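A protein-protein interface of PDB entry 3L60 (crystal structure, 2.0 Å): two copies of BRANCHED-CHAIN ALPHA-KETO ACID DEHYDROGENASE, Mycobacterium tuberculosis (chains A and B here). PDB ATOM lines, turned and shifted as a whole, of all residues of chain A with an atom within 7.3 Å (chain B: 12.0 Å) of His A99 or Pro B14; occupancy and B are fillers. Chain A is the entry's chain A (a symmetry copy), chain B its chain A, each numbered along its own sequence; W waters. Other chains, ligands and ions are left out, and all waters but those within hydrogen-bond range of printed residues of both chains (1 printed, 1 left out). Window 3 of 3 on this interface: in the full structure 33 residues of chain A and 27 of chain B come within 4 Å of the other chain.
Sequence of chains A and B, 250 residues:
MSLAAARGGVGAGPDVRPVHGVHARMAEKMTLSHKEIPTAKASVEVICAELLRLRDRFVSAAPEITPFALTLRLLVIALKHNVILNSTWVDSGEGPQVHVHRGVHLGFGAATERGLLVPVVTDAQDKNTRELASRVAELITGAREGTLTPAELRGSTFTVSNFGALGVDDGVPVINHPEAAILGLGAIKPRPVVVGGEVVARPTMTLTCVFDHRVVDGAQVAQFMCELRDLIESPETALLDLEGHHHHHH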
ATOM      1  N   VAL A  83      -8.752  10.546  21.604  1.00  0.00           N
ATOM      2  CA  VAL A  83      -9.855   9.798  22.197  1.00  0.00           C
ATOM      3  C   VAL A  83     -11.169  10.535  22.232  1.00  0.00           C
ATOM      4  O   VAL A  83     -12.230   9.894  22.179  1.00  0.00           O
ATOM      5  CB  VAL A  83      -9.504   9.203  23.613  1.00  0.00           C
ATOM      6  CG1 VAL A  83      -8.382   8.150  23.473  1.00  0.00           C
ATOM      7  CG2 VAL A  83      -9.109  10.270  24.588  1.00  0.00           C
ATOM      8  N   ILE A  84     -11.114  11.874  22.279  1.00  0.00           N
ATOM      9  CA  ILE A  84     -12.299  12.699  22.343  1.00  0.00           C
ATOM     10  C   ILE A  84     -13.198  12.556  21.084  1.00  0.00           C
ATOM     11  O   ILE A  84     -14.434  12.839  21.148  1.00  0.00           O
ATOM     12  CB  ILE A  84     -11.932  14.183  22.594  1.00  0.00           C
ATOM     13  CG1 ILE A  84     -13.132  15.017  23.031  1.00  0.00           C
ATOM     14  CG2 ILE A  84     -11.256  14.832  21.348  1.00  0.00           C
ATOM     15  CD1 ILE A  84     -13.713  14.701  24.369  1.00  0.00           C
ATOM     16  N   ASN A  86     -14.084   9.844  19.770  1.00  0.00           N
ATOM     17  CA  ASN A  86     -14.810   8.587  19.902  1.00  0.00           C
ATOM     18  C   ASN A  86     -15.528   8.652  21.232  1.00  0.00           C
ATOM     19  O   ASN A  86     -15.075   8.125  22.212  1.00  0.00           O
ATOM     20  CB  ASN A  86     -13.826   7.423  19.836  1.00  0.00           C
ATOM     21  CG  ASN A  86     -14.497   6.076  19.678  1.00  0.00           C
ATOM     22  OD1 ASN A  86     -15.043   5.769  18.662  1.00  0.00           O
ATOM     23  ND2 ASN A  86     -14.392   5.263  20.683  1.00  0.00           N
ATOM     24  N   SER A  87     -16.647   9.353  21.252  1.00  0.00           N
ATOM     25  CA  SER A  87     -17.287   9.760  22.485  1.00  0.00           C
ATOM     26  C   SER A  87     -18.753  10.144  22.279  1.00  0.00           C
ATOM     27  O   SER A  87     -19.268  10.134  21.148  1.00  0.00           O
ATOM     28  CB  SER A  87     -16.502  10.937  23.090  1.00  0.00           C
ATOM     29  OG  SER A  87     -16.586  12.060  22.235  1.00  0.00           O
ATOM     30  N   THR A  88     -19.428  10.488  23.368  1.00  0.00           N
ATOM     31  CA  THR A  88     -20.841  10.808  23.337  1.00  0.00           C
ATOM     32  C   THR A  88     -21.148  11.935  24.318  1.00  0.00           C
ATOM     33  O   THR A  88     -20.643  11.939  25.453  1.00  0.00           O
ATOM     34  CB  THR A  88     -21.732   9.577  23.710  1.00  0.00           C
ATOM     35  OG1 THR A  88     -21.569   8.510  22.755  1.00  0.00           O
ATOM     36  CG2 THR A  88     -23.201   9.975  23.739  1.00  0.00           C
ATOM     37  N   TRP A  89     -21.976  12.878  23.886  1.00  0.00           N
ATOM     38  CA  TRP A  89     -22.459  13.943  24.778  1.00  0.00           C
ATOM     39  C   TRP A  89     -23.606  13.367  25.620  1.00  0.00           C
ATOM     40  O   TRP A  89     -24.522  12.755  25.084  1.00  0.00           O
ATOM     41  CB  TRP A  89     -22.942  15.161  23.982  1.00  0.00           C
ATOM     42  CG  TRP A  89     -23.524  16.292  24.827  1.00  0.00           C
ATOM     43  CD1 TRP A  89     -24.840  16.494  25.127  1.00  0.00           C
ATOM     44  CD2 TRP A  89     -22.801  17.352  25.472  1.00  0.00           C
ATOM     45  NE1 TRP A  89     -24.984  17.612  25.911  1.00  0.00           N
ATOM     46  CE2 TRP A  89     -23.750  18.164  26.130  1.00  0.00           C
ATOM     47  CE3 TRP A  89     -21.450  17.703  25.544  1.00  0.00           C
ATOM     48  CZ2 TRP A  89     -23.384  19.290  26.873  1.00  0.00           C
ATOM     49  CZ3 TRP A  89     -21.089  18.844  26.269  1.00  0.00           C
ATOM     50  CH2 TRP A  89     -22.047  19.609  26.921  1.00  0.00           C
ATOM     51  N   VAL A  90     -23.546  13.585  26.925  1.00  0.00           N
ATOM     52  CA  VAL A  90     -24.574  13.070  27.841  1.00  0.00           C
ATOM     53  C   VAL A  90     -25.040  14.185  28.771  1.00  0.00           C
ATOM     54  O   VAL A  90     -24.209  14.898  29.371  1.00  0.00           O
ATOM     55  CB  VAL A  90     -24.042  11.865  28.649  1.00  0.00           C
ATOM     56  CG1 VAL A  90     -25.035  11.483  29.760  1.00  0.00           C
ATOM     57  CG2 VAL A  90     -23.780  10.677  27.724  1.00  0.00           C
ATOM     58  N   ASP A  91     -26.363  14.360  28.846  1.00  0.00           N
ATOM     59  CA  ASP A  91     -26.982  15.334  29.769  1.00  0.00           C
ATOM     60  C   ASP A  91     -27.850  14.682  30.854  1.00  0.00           C
ATOM     61  O   ASP A  91     -28.070  15.278  31.920  1.00  0.00           O
ATOM     62  CB  ASP A  91     -27.824  16.356  29.001  1.00  0.00           C
ATOM     63  CG  ASP A  91     -27.416  17.789  29.314  1.00  0.00           C
ATOM     64  OD1 ASP A  91     -27.352  18.595  28.360  1.00  0.00           O
ATOM     65  OD2 ASP A  91     -27.122  18.097  30.497  1.00  0.00           O
ATOM     66  N   SER A  92     -28.349  13.477  30.575  1.00  0.00           N
ATOM     67  CA  SER A  92     -29.056  12.660  31.558  1.00  0.00           C
ATOM     68  C   SER A  92     -28.352  12.654  32.918  1.00  0.00           C
ATOM     69  O   SER A  92     -27.202  12.191  33.026  1.00  0.00           O
ATOM     70  CB  SER A  92     -29.175  11.216  31.054  1.00  0.00           C
ATOM     71  N   PRO A  96     -23.891  18.291  32.452  1.00  0.00           N
ATOM     72  CA  PRO A  96     -23.245  17.934  31.191  1.00  0.00           C
ATOM     73  C   PRO A  96     -21.966  17.127  31.377  1.00  0.00           C
ATOM     74  O   PRO A  96     -21.052  17.544  32.132  1.00  0.00           O
ATOM     75  CB  PRO A  96     -22.914  19.292  30.567  1.00  0.00           C
ATOM     76  CG  PRO A  96     -22.790  20.212  31.724  1.00  0.00           C
ATOM     77  CD  PRO A  96     -23.880  19.748  32.655  1.00  0.00           C
ATOM     78  N   GLN A  97     -21.914  15.999  30.656  1.00  0.00           N
ATOM     79  CA  GLN A  97     -20.769  15.072  30.638  1.00  0.00           C
ATOM     80  C   GLN A  97     -20.408  14.635  29.203  1.00  0.00           C
ATOM     81  O   GLN A  97     -21.275  14.510  28.344  1.00  0.00           O
ATOM     82  CB  GLN A  97     -21.102  13.803  31.425  1.00  0.00           C
ATOM     83  CG  GLN A  97     -21.294  14.004  32.922  1.00  0.00           C
ATOM     84  CD  GLN A  97     -22.046  12.863  33.576  1.00  0.00           C
ATOM     85  OE1 GLN A  97     -22.643  12.011  32.907  1.00  0.00           O
ATOM     86  NE2 GLN A  97     -22.033  12.848  34.908  1.00  0.00           N
ATOM     87  N   VAL A  98     -19.129  14.395  28.972  1.00  0.00           N
ATOM     88  CA  VAL A  98     -18.665  13.715  27.767  1.00  0.00           C
ATOM     89  C   VAL A  98     -18.244  12.318  28.205  1.00  0.00           C
ATOM     90  O   VAL A  98     -17.375  12.171  29.088  1.00  0.00           O
ATOM     91  CB  VAL A  98     -17.466  14.456  27.162  1.00  0.00           C
ATOM     92  CG1 VAL A  98     -16.826  13.663  26.053  1.00  0.00           C
ATOM     93  CG2 VAL A  98     -17.906  15.866  26.689  1.00  0.00           C
ATOM     94  N   HIS A  99     -18.856  11.300  27.610  1.00  0.00           N
ATOM     95  CA  HIS A  99     -18.437   9.910  27.824  1.00  0.00           C
ATOM     96  C   HIS A  99     -17.472   9.489  26.737  1.00  0.00           C
ATOM     97  O   HIS A  99     -17.865   9.359  25.573  1.00  0.00           O
ATOM     98  CB  HIS A  99     -19.664   9.002  27.835  1.00  0.00           C
ATOM     99  CG  HIS A  99     -20.534   9.191  29.044  1.00  0.00           C
ATOM    100  ND1 HIS A  99     -21.401   8.222  29.503  1.00  0.00           N
ATOM    101  CD2 HIS A  99     -20.628  10.220  29.918  1.00  0.00           C
ATOM    102  CE1 HIS A  99     -22.014   8.661  30.587  1.00  0.00           C
ATOM    103  NE2 HIS A  99     -21.559   9.868  30.864  1.00  0.00           N
ATOM    104  N   VAL A 100     -16.214   9.272  27.108  1.00  0.00           N
ATOM    105  CA  VAL A 100     -15.177   8.847  26.183  1.00  0.00           C
ATOM    106  C   VAL A 100     -15.088   7.314  26.181  1.00  0.00           C
ATOM    107  O   VAL A 100     -14.848   6.686  27.227  1.00  0.00           O
ATOM    108  CB  VAL A 100     -13.842   9.517  26.526  1.00  0.00           C
ATOM    109  CG1 VAL A 100     -12.734   8.994  25.671  1.00  0.00           C
ATOM    110  CG2 VAL A 100     -13.972  11.059  26.414  1.00  0.00           C
ATOM    111  N   HIS A 101     -15.322   6.709  25.015  1.00  0.00           N
ATOM    112  CA  HIS A 101     -15.443   5.250  24.909  1.00  0.00           C
ATOM    113  C   HIS A 101     -14.100   4.570  24.757  1.00  0.00           C
ATOM    114  O   HIS A 101     -13.288   5.004  23.947  1.00  0.00           O
ATOM    115  CB  HIS A 101     -16.325   4.860  23.725  1.00  0.00           C
ATOM    116  CG  HIS A 101     -17.691   5.445  23.784  1.00  0.00           C
ATOM    117  ND1 HIS A 101     -18.560   5.193  24.821  1.00  0.00           N
ATOM    118  CD2 HIS A 101     -18.335   6.289  22.944  1.00  0.00           C
ATOM    119  CE1 HIS A 101     -19.680   5.870  24.624  1.00  0.00           C
ATOM    120  NE2 HIS A 101     -19.569   6.534  23.487  1.00  0.00           N
ATOM    121  N   ARG A 102     -13.900   3.456  25.467  1.00  0.00           N
ATOM    122  CA  ARG A 102     -12.607   2.774  25.450  1.00  0.00           C
ATOM    123  C   ARG A 102     -12.480   1.896  24.198  1.00  0.00           C
ATOM    124  O   ARG A 102     -11.402   1.758  23.623  1.00  0.00           O
ATOM    125  CB  ARG A 102     -12.376   1.917  26.718  1.00  0.00           C
ATOM    126  CG  ARG A 102     -13.378   2.127  27.886  1.00  0.00           C
ATOM    127  CD  ARG A 102     -12.746   1.958  29.299  1.00  0.00           C
ATOM    128  NE  ARG A 102     -12.023   3.174  29.706  1.00  0.00           N
ATOM    129  CZ  ARG A 102     -12.033   3.721  30.927  1.00  0.00           C
ATOM    130  NH1 ARG A 102     -12.734   3.190  31.926  1.00  0.00           N
ATOM    131  NH2 ARG A 102     -11.331   4.824  31.147  1.00  0.00           N
ATOM    132  N   PRO A 178     -25.826   8.500  18.957  1.00  0.00           N
ATOM    133  CA  PRO A 178     -25.264   9.554  19.812  1.00  0.00           C
ATOM    134  C   PRO A 178     -23.723   9.706  19.698  1.00  0.00           C
ATOM    135  O   PRO A 178     -23.050  10.079  20.660  1.00  0.00           O
ATOM    136  CB  PRO A 178     -25.613   9.049  21.217  1.00  0.00           C
ATOM    137  CG  PRO A 178     -25.416   7.584  21.101  1.00  0.00           C
ATOM    138  CD  PRO A 178     -25.836   7.209  19.678  1.00  0.00           C
ATOM    139  N   ALA A 180     -20.084  11.386  18.465  1.00  0.00           N
ATOM    140  CA  ALA A 180     -19.582  12.757  18.503  1.00  0.00           C
ATOM    141  C   ALA A 180     -19.028  13.246  17.147  1.00  0.00           C
ATOM    142  O   ALA A 180     -18.804  14.430  16.977  1.00  0.00           O
ATOM    143  CB  ALA A 180     -18.501  12.884  19.574  1.00  0.00           C
ATOM    144  N   VAL A 215     -18.760  18.680  22.064  1.00  0.00           N
ATOM    145  CA  VAL A 215     -17.852  17.633  22.536  1.00  0.00           C
ATOM    146  C   VAL A 215     -16.415  17.939  22.124  1.00  0.00           C
ATOM    147  O   VAL A 215     -15.501  17.981  22.971  1.00  0.00           O
ATOM    148  CB  VAL A 215     -18.287  16.282  21.960  1.00  0.00           C
ATOM    149  CG1 VAL A 215     -17.331  15.148  22.351  1.00  0.00           C
ATOM    150  CG2 VAL A 215     -19.666  15.967  22.427  1.00  0.00           C
ATOM    151  N   PRO B  14     -17.445   3.697  30.115  1.00  0.00           N
ATOM    152  CA  PRO B  14     -16.699   4.821  29.495  1.00  0.00           C
ATOM    153  C   PRO B  14     -16.007   5.750  30.516  1.00  0.00           C
ATOM    154  O   PRO B  14     -16.443   5.845  31.662  1.00  0.00           O
ATOM    155  CB  PRO B  14     -17.787   5.577  28.694  1.00  0.00           C
ATOM    156  CG  PRO B  14     -19.124   5.201  29.352  1.00  0.00           C
ATOM    157  CD  PRO B  14     -18.910   3.800  29.943  1.00  0.00           C
ATOM    158  N   ASP B  15     -14.920   6.399  30.107  1.00  0.00           N
ATOM    159  CA  ASP B  15     -14.314   7.499  30.871  1.00  0.00           C
ATOM    160  C   ASP B  15     -15.268   8.735  30.881  1.00  0.00           C
ATOM    161  O   ASP B  15     -15.498   9.383  29.844  1.00  0.00           O
ATOM    162  CB  ASP B  15     -12.935   7.812  30.268  1.00  0.00           C
ATOM    163  CG  ASP B  15     -12.305   9.088  30.808  1.00  0.00           C
ATOM    164  OD1 ASP B  15     -12.781   9.671  31.815  1.00  0.00           O
ATOM    165  OD2 ASP B  15     -11.309   9.520  30.197  1.00  0.00           O
ATOM    166  N   VAL B  16     -15.823   9.051  32.051  1.00  0.00           N
ATOM    167  CA  VAL B  16     -16.847  10.084  32.167  1.00  0.00           C
ATOM    168  C   VAL B  16     -16.224  11.409  32.543  1.00  0.00           C
ATOM    169  O   VAL B  16     -15.640  11.531  33.618  1.00  0.00           O
ATOM    170  CB  VAL B  16     -17.891   9.730  33.220  1.00  0.00           C
ATOM    171  CG1 VAL B  16     -18.843  10.912  33.446  1.00  0.00           C
ATOM    172  CG2 VAL B  16     -18.644   8.489  32.809  1.00  0.00           C
ATOM    173  N   ARG B  17     -16.335  12.402  31.659  1.00  0.00           N
ATOM    174  CA  ARG B  17     -15.713  13.705  31.903  1.00  0.00           C
ATOM    175  C   ARG B  17     -16.785  14.749  32.151  1.00  0.00           C
ATOM    176  O   ARG B  17     -17.557  15.070  31.244  1.00  0.00           O
ATOM    177  CB  ARG B  17     -14.842  14.111  30.726  1.00  0.00           C
ATOM    178  CG  ARG B  17     -13.878  13.040  30.374  1.00  0.00           C
ATOM    179  CD  ARG B  17     -12.929  13.472  29.329  1.00  0.00           C
ATOM    180  NE  ARG B  17     -11.978  12.415  29.046  1.00  0.00           N
ATOM    181  CZ  ARG B  17     -10.990  12.514  28.166  1.00  0.00           C
ATOM    182  NH1 ARG B  17     -10.811  13.626  27.465  1.00  0.00           N
ATOM    183  NH2 ARG B  17     -10.178  11.485  27.986  1.00  0.00           N
ATOM    184  N   PRO B  18     -16.879  15.262  33.396  1.00  0.00           N
ATOM    185  CA  PRO B  18     -17.844  16.346  33.621  1.00  0.00           C
ATOM    186  C   PRO B  18     -17.380  17.577  32.862  1.00  0.00           C
ATOM    187  O   PRO B  18     -16.182  17.778  32.715  1.00  0.00           O
ATOM    188  CB  PRO B  18     -17.781  16.569  35.148  1.00  0.00           C
ATOM    189  CG  PRO B  18     -17.236  15.282  35.700  1.00  0.00           C
ATOM    190  CD  PRO B  18     -16.247  14.826  34.654  1.00  0.00           C
ATOM    191  N   VAL B  19     -18.306  18.383  32.371  1.00  0.00           N
ATOM    192  CA  VAL B  19     -17.943  19.549  31.547  1.00  0.00           C
ATOM    193  C   VAL B  19     -18.085  20.860  32.372  1.00  0.00           C
ATOM    194  O   VAL B  19     -19.150  21.113  32.937  1.00  0.00           O
ATOM    195  CB  VAL B  19     -18.834  19.580  30.264  1.00  0.00           C
ATOM    196  CG1 VAL B  19     -18.485  20.774  29.361  1.00  0.00           C
ATOM    197  CG2 VAL B  19     -18.721  18.246  29.489  1.00  0.00           C
ATOM    198  N   HIS B  20     -17.014  21.666  32.441  1.00  0.00           N
ATOM    199  CA  HIS B  20     -17.054  22.987  33.120  1.00  0.00           C
ATOM    200  C   HIS B  20     -16.329  24.096  32.337  1.00  0.00           C
ATOM    201  O   HIS B  20     -15.640  23.851  31.341  1.00  0.00           O
ATOM    202  CB  HIS B  20     -16.389  22.946  34.514  1.00  0.00           C
ATOM    203  CG  HIS B  20     -16.764  21.777  35.367  1.00  0.00           C
ATOM    204  ND1 HIS B  20     -17.931  21.731  36.097  1.00  0.00           N
ATOM    205  CD2 HIS B  20     -16.091  20.635  35.659  1.00  0.00           C
ATOM    206  CE1 HIS B  20     -17.975  20.601  36.784  1.00  0.00           C
ATOM    207  NE2 HIS B  20     -16.867  19.921  36.542  1.00  0.00           N
ATOM    208  N   HIS B  23     -15.112  24.914  28.320  1.00  0.00           N
ATOM    209  CA  HIS B  23     -15.836  23.836  27.632  1.00  0.00           C
ATOM    210  C   HIS B  23     -17.364  23.986  27.780  1.00  0.00           C
ATOM    211  O   HIS B  23     -18.096  23.904  26.778  1.00  0.00           O
ATOM    212  CB  HIS B  23     -15.378  22.456  28.127  1.00  0.00           C
ATOM    213  CG  HIS B  23     -15.744  21.322  27.207  1.00  0.00           C
ATOM    214  ND1 HIS B  23     -15.043  20.135  27.181  1.00  0.00           N
ATOM    215  CD2 HIS B  23     -16.730  21.194  26.282  1.00  0.00           C
ATOM    216  CE1 HIS B  23     -15.579  19.328  26.282  1.00  0.00           C
ATOM    217  NE2 HIS B  23     -16.598  19.951  25.717  1.00  0.00           N
ATOM    218  N   ALA B  27     -19.922  24.660  24.704  1.00  0.00           N
ATOM    219  CA  ALA B  27     -21.100  23.782  24.583  1.00  0.00           C
ATOM    220  C   ALA B  27     -22.446  24.557  24.627  1.00  0.00           C
ATOM    221  O   ALA B  27     -23.366  24.265  23.853  1.00  0.00           O
ATOM    222  CB  ALA B  27     -21.067  22.674  25.674  1.00  0.00           C
HETATM  223  O   HOH W   1     -20.513  19.293  34.607  1.00  0.00           O
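Among the printed residues, pairs that only touch across the chains: Gln A97 with Arg B17 (3.3 Å), Trp A89 with Ala B27 (3.5 Å), Val A100 with Pro B14 (3.5 Å), Arg A102 with Asp B15 (3.5 Å), Val A215 with His B23 (3.6 Å), Val A100 with Arg B17 (3.6 Å), His A99 with Asp B15 (3.6 Å), Val A98 with Val B16 (3.7 Å), Pro A96 with Pro B18 (3.7 Å), Gln A97 with Val B16 (3.8 Å), Val A83 with Arg B17 (3.8 Å), Val A98 with Val B19 (3.8 Å), His A99 with Val B16 (3.8 Å), His A99 with Pro B14 (3.8 Å), Gln A97 with Val B19 (3.9 Å) and His A101 with Pro B14 (3.97 Å).
The guanidinium group (NH2) of Arg B17 lies within salt-bridge range of the side-chain carboxylate (OD2) of Asp B15 (3.2 Å).
O of Asn A86 sits at hydrogen-bond distance from N of His A101 (3.2 Å).
The backbone carbonyl oxygen (O) of Thr A88 is in hydrogen-bond range of the backbone NH (N) of His A99 (2.9 Å).
The side-chain hydroxyl (OG1) of Thr A88 is in hydrogen-bond range of a ring nitrogen (NE2) of His A101, 2.9 Å away.
The backbone carbonyl oxygen (O) of Gln A97 is in hydrogen-bond range of the backbone NH (N) of Val A90, 2.8 Å away.
OE1 of Gln A97 sits at hydrogen-bond distance from NE2 of His A99 (3.2 Å).
His A99 touches three residues of chain B.
Printed residues of chain A within 4 Å of Pro B14: His A99 (3.8 Å), Val A100 (3.5 Å) and His A101 (3.97 Å).
No residue of chain B comes within 4 Å of Ser A87.
No residue of chain B comes within 4 Å of Thr A88.
Gln A97 touches three residues of chain B.
His A101 touches one residue of chain B.
Of the printed residues of chain B, Trp A89 touches Ala B27 (3.5 Å).
Printed residues of chain B within 4 Å of Pro A96: Pro B18 and Val B19.
Printed residues of chain B within 4 Å of Arg A102: Asp B15.
Printed residues of chain A within 4 Å of Ala B27: Trp A89 (3.5 Å).
Of the printed residues of chain A, Val B19 touches Pro A96 (2.9 Å), Gln A97 (3.9 Å) and Val A98 (3.8 Å).
His B20 touches none of the printed residues of chain A.
The nearest residue of chain B that does not touch His A99 is Arg B17 (4.9 Å).
The nearest printed residue of chain A that does not touch Ala B27 is Val A215 (5.9 Å).
No position is printed for both chains.
Of the 20 pairs that touch across the chains among the printed residues, none has its exchanged pair printed and touching as well.
Of the 9 printed residues of chain B, 8 touch a printed residue of chain A.
Hydrophobic or aromatic side chains of chain B within 4 Å of the printed part of chain A: Pro B14, Val B16, Val B19, His B23 and Ala B27.
Along chain B the printed residues that touch a printed residue of chain A span positions 14 to 27.
Of the 19 printed residues of chain A, 10 touch a printed residue of chain B.
Hydrophobic or aromatic side chains of chain A within 4 Å of the printed part of chain B: Val A83, Trp A89, Pro A96, Val A98, His A99, Val A100 and His A101.
Among the printed residues, no Asp or Glu carboxylate lies within 4 Å of a Lys or Arg side-chain nitrogen of the other chain.
N of Val A100 is in hydrogen-bond range of O of Asp B15 (2.8 Å).
N of Arg B17 is in hydrogen-bond range of O of Val A98 (2.8 Å).
The backbone carbonyl oxygen (O) of Pro A96 lies within hydrogen-bond range of the backbone NH (N) of Val B19.
The backbone carbonyl oxygen (O) of Val A98 sits close to the backbone carbonyl oxygen (O) of Asp B15, at 3.4 Å.
Water W1 lies within hydrogen-bond range of O of Val B19 (2.8 Å) and O of Pro A96 (3.1 Å).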
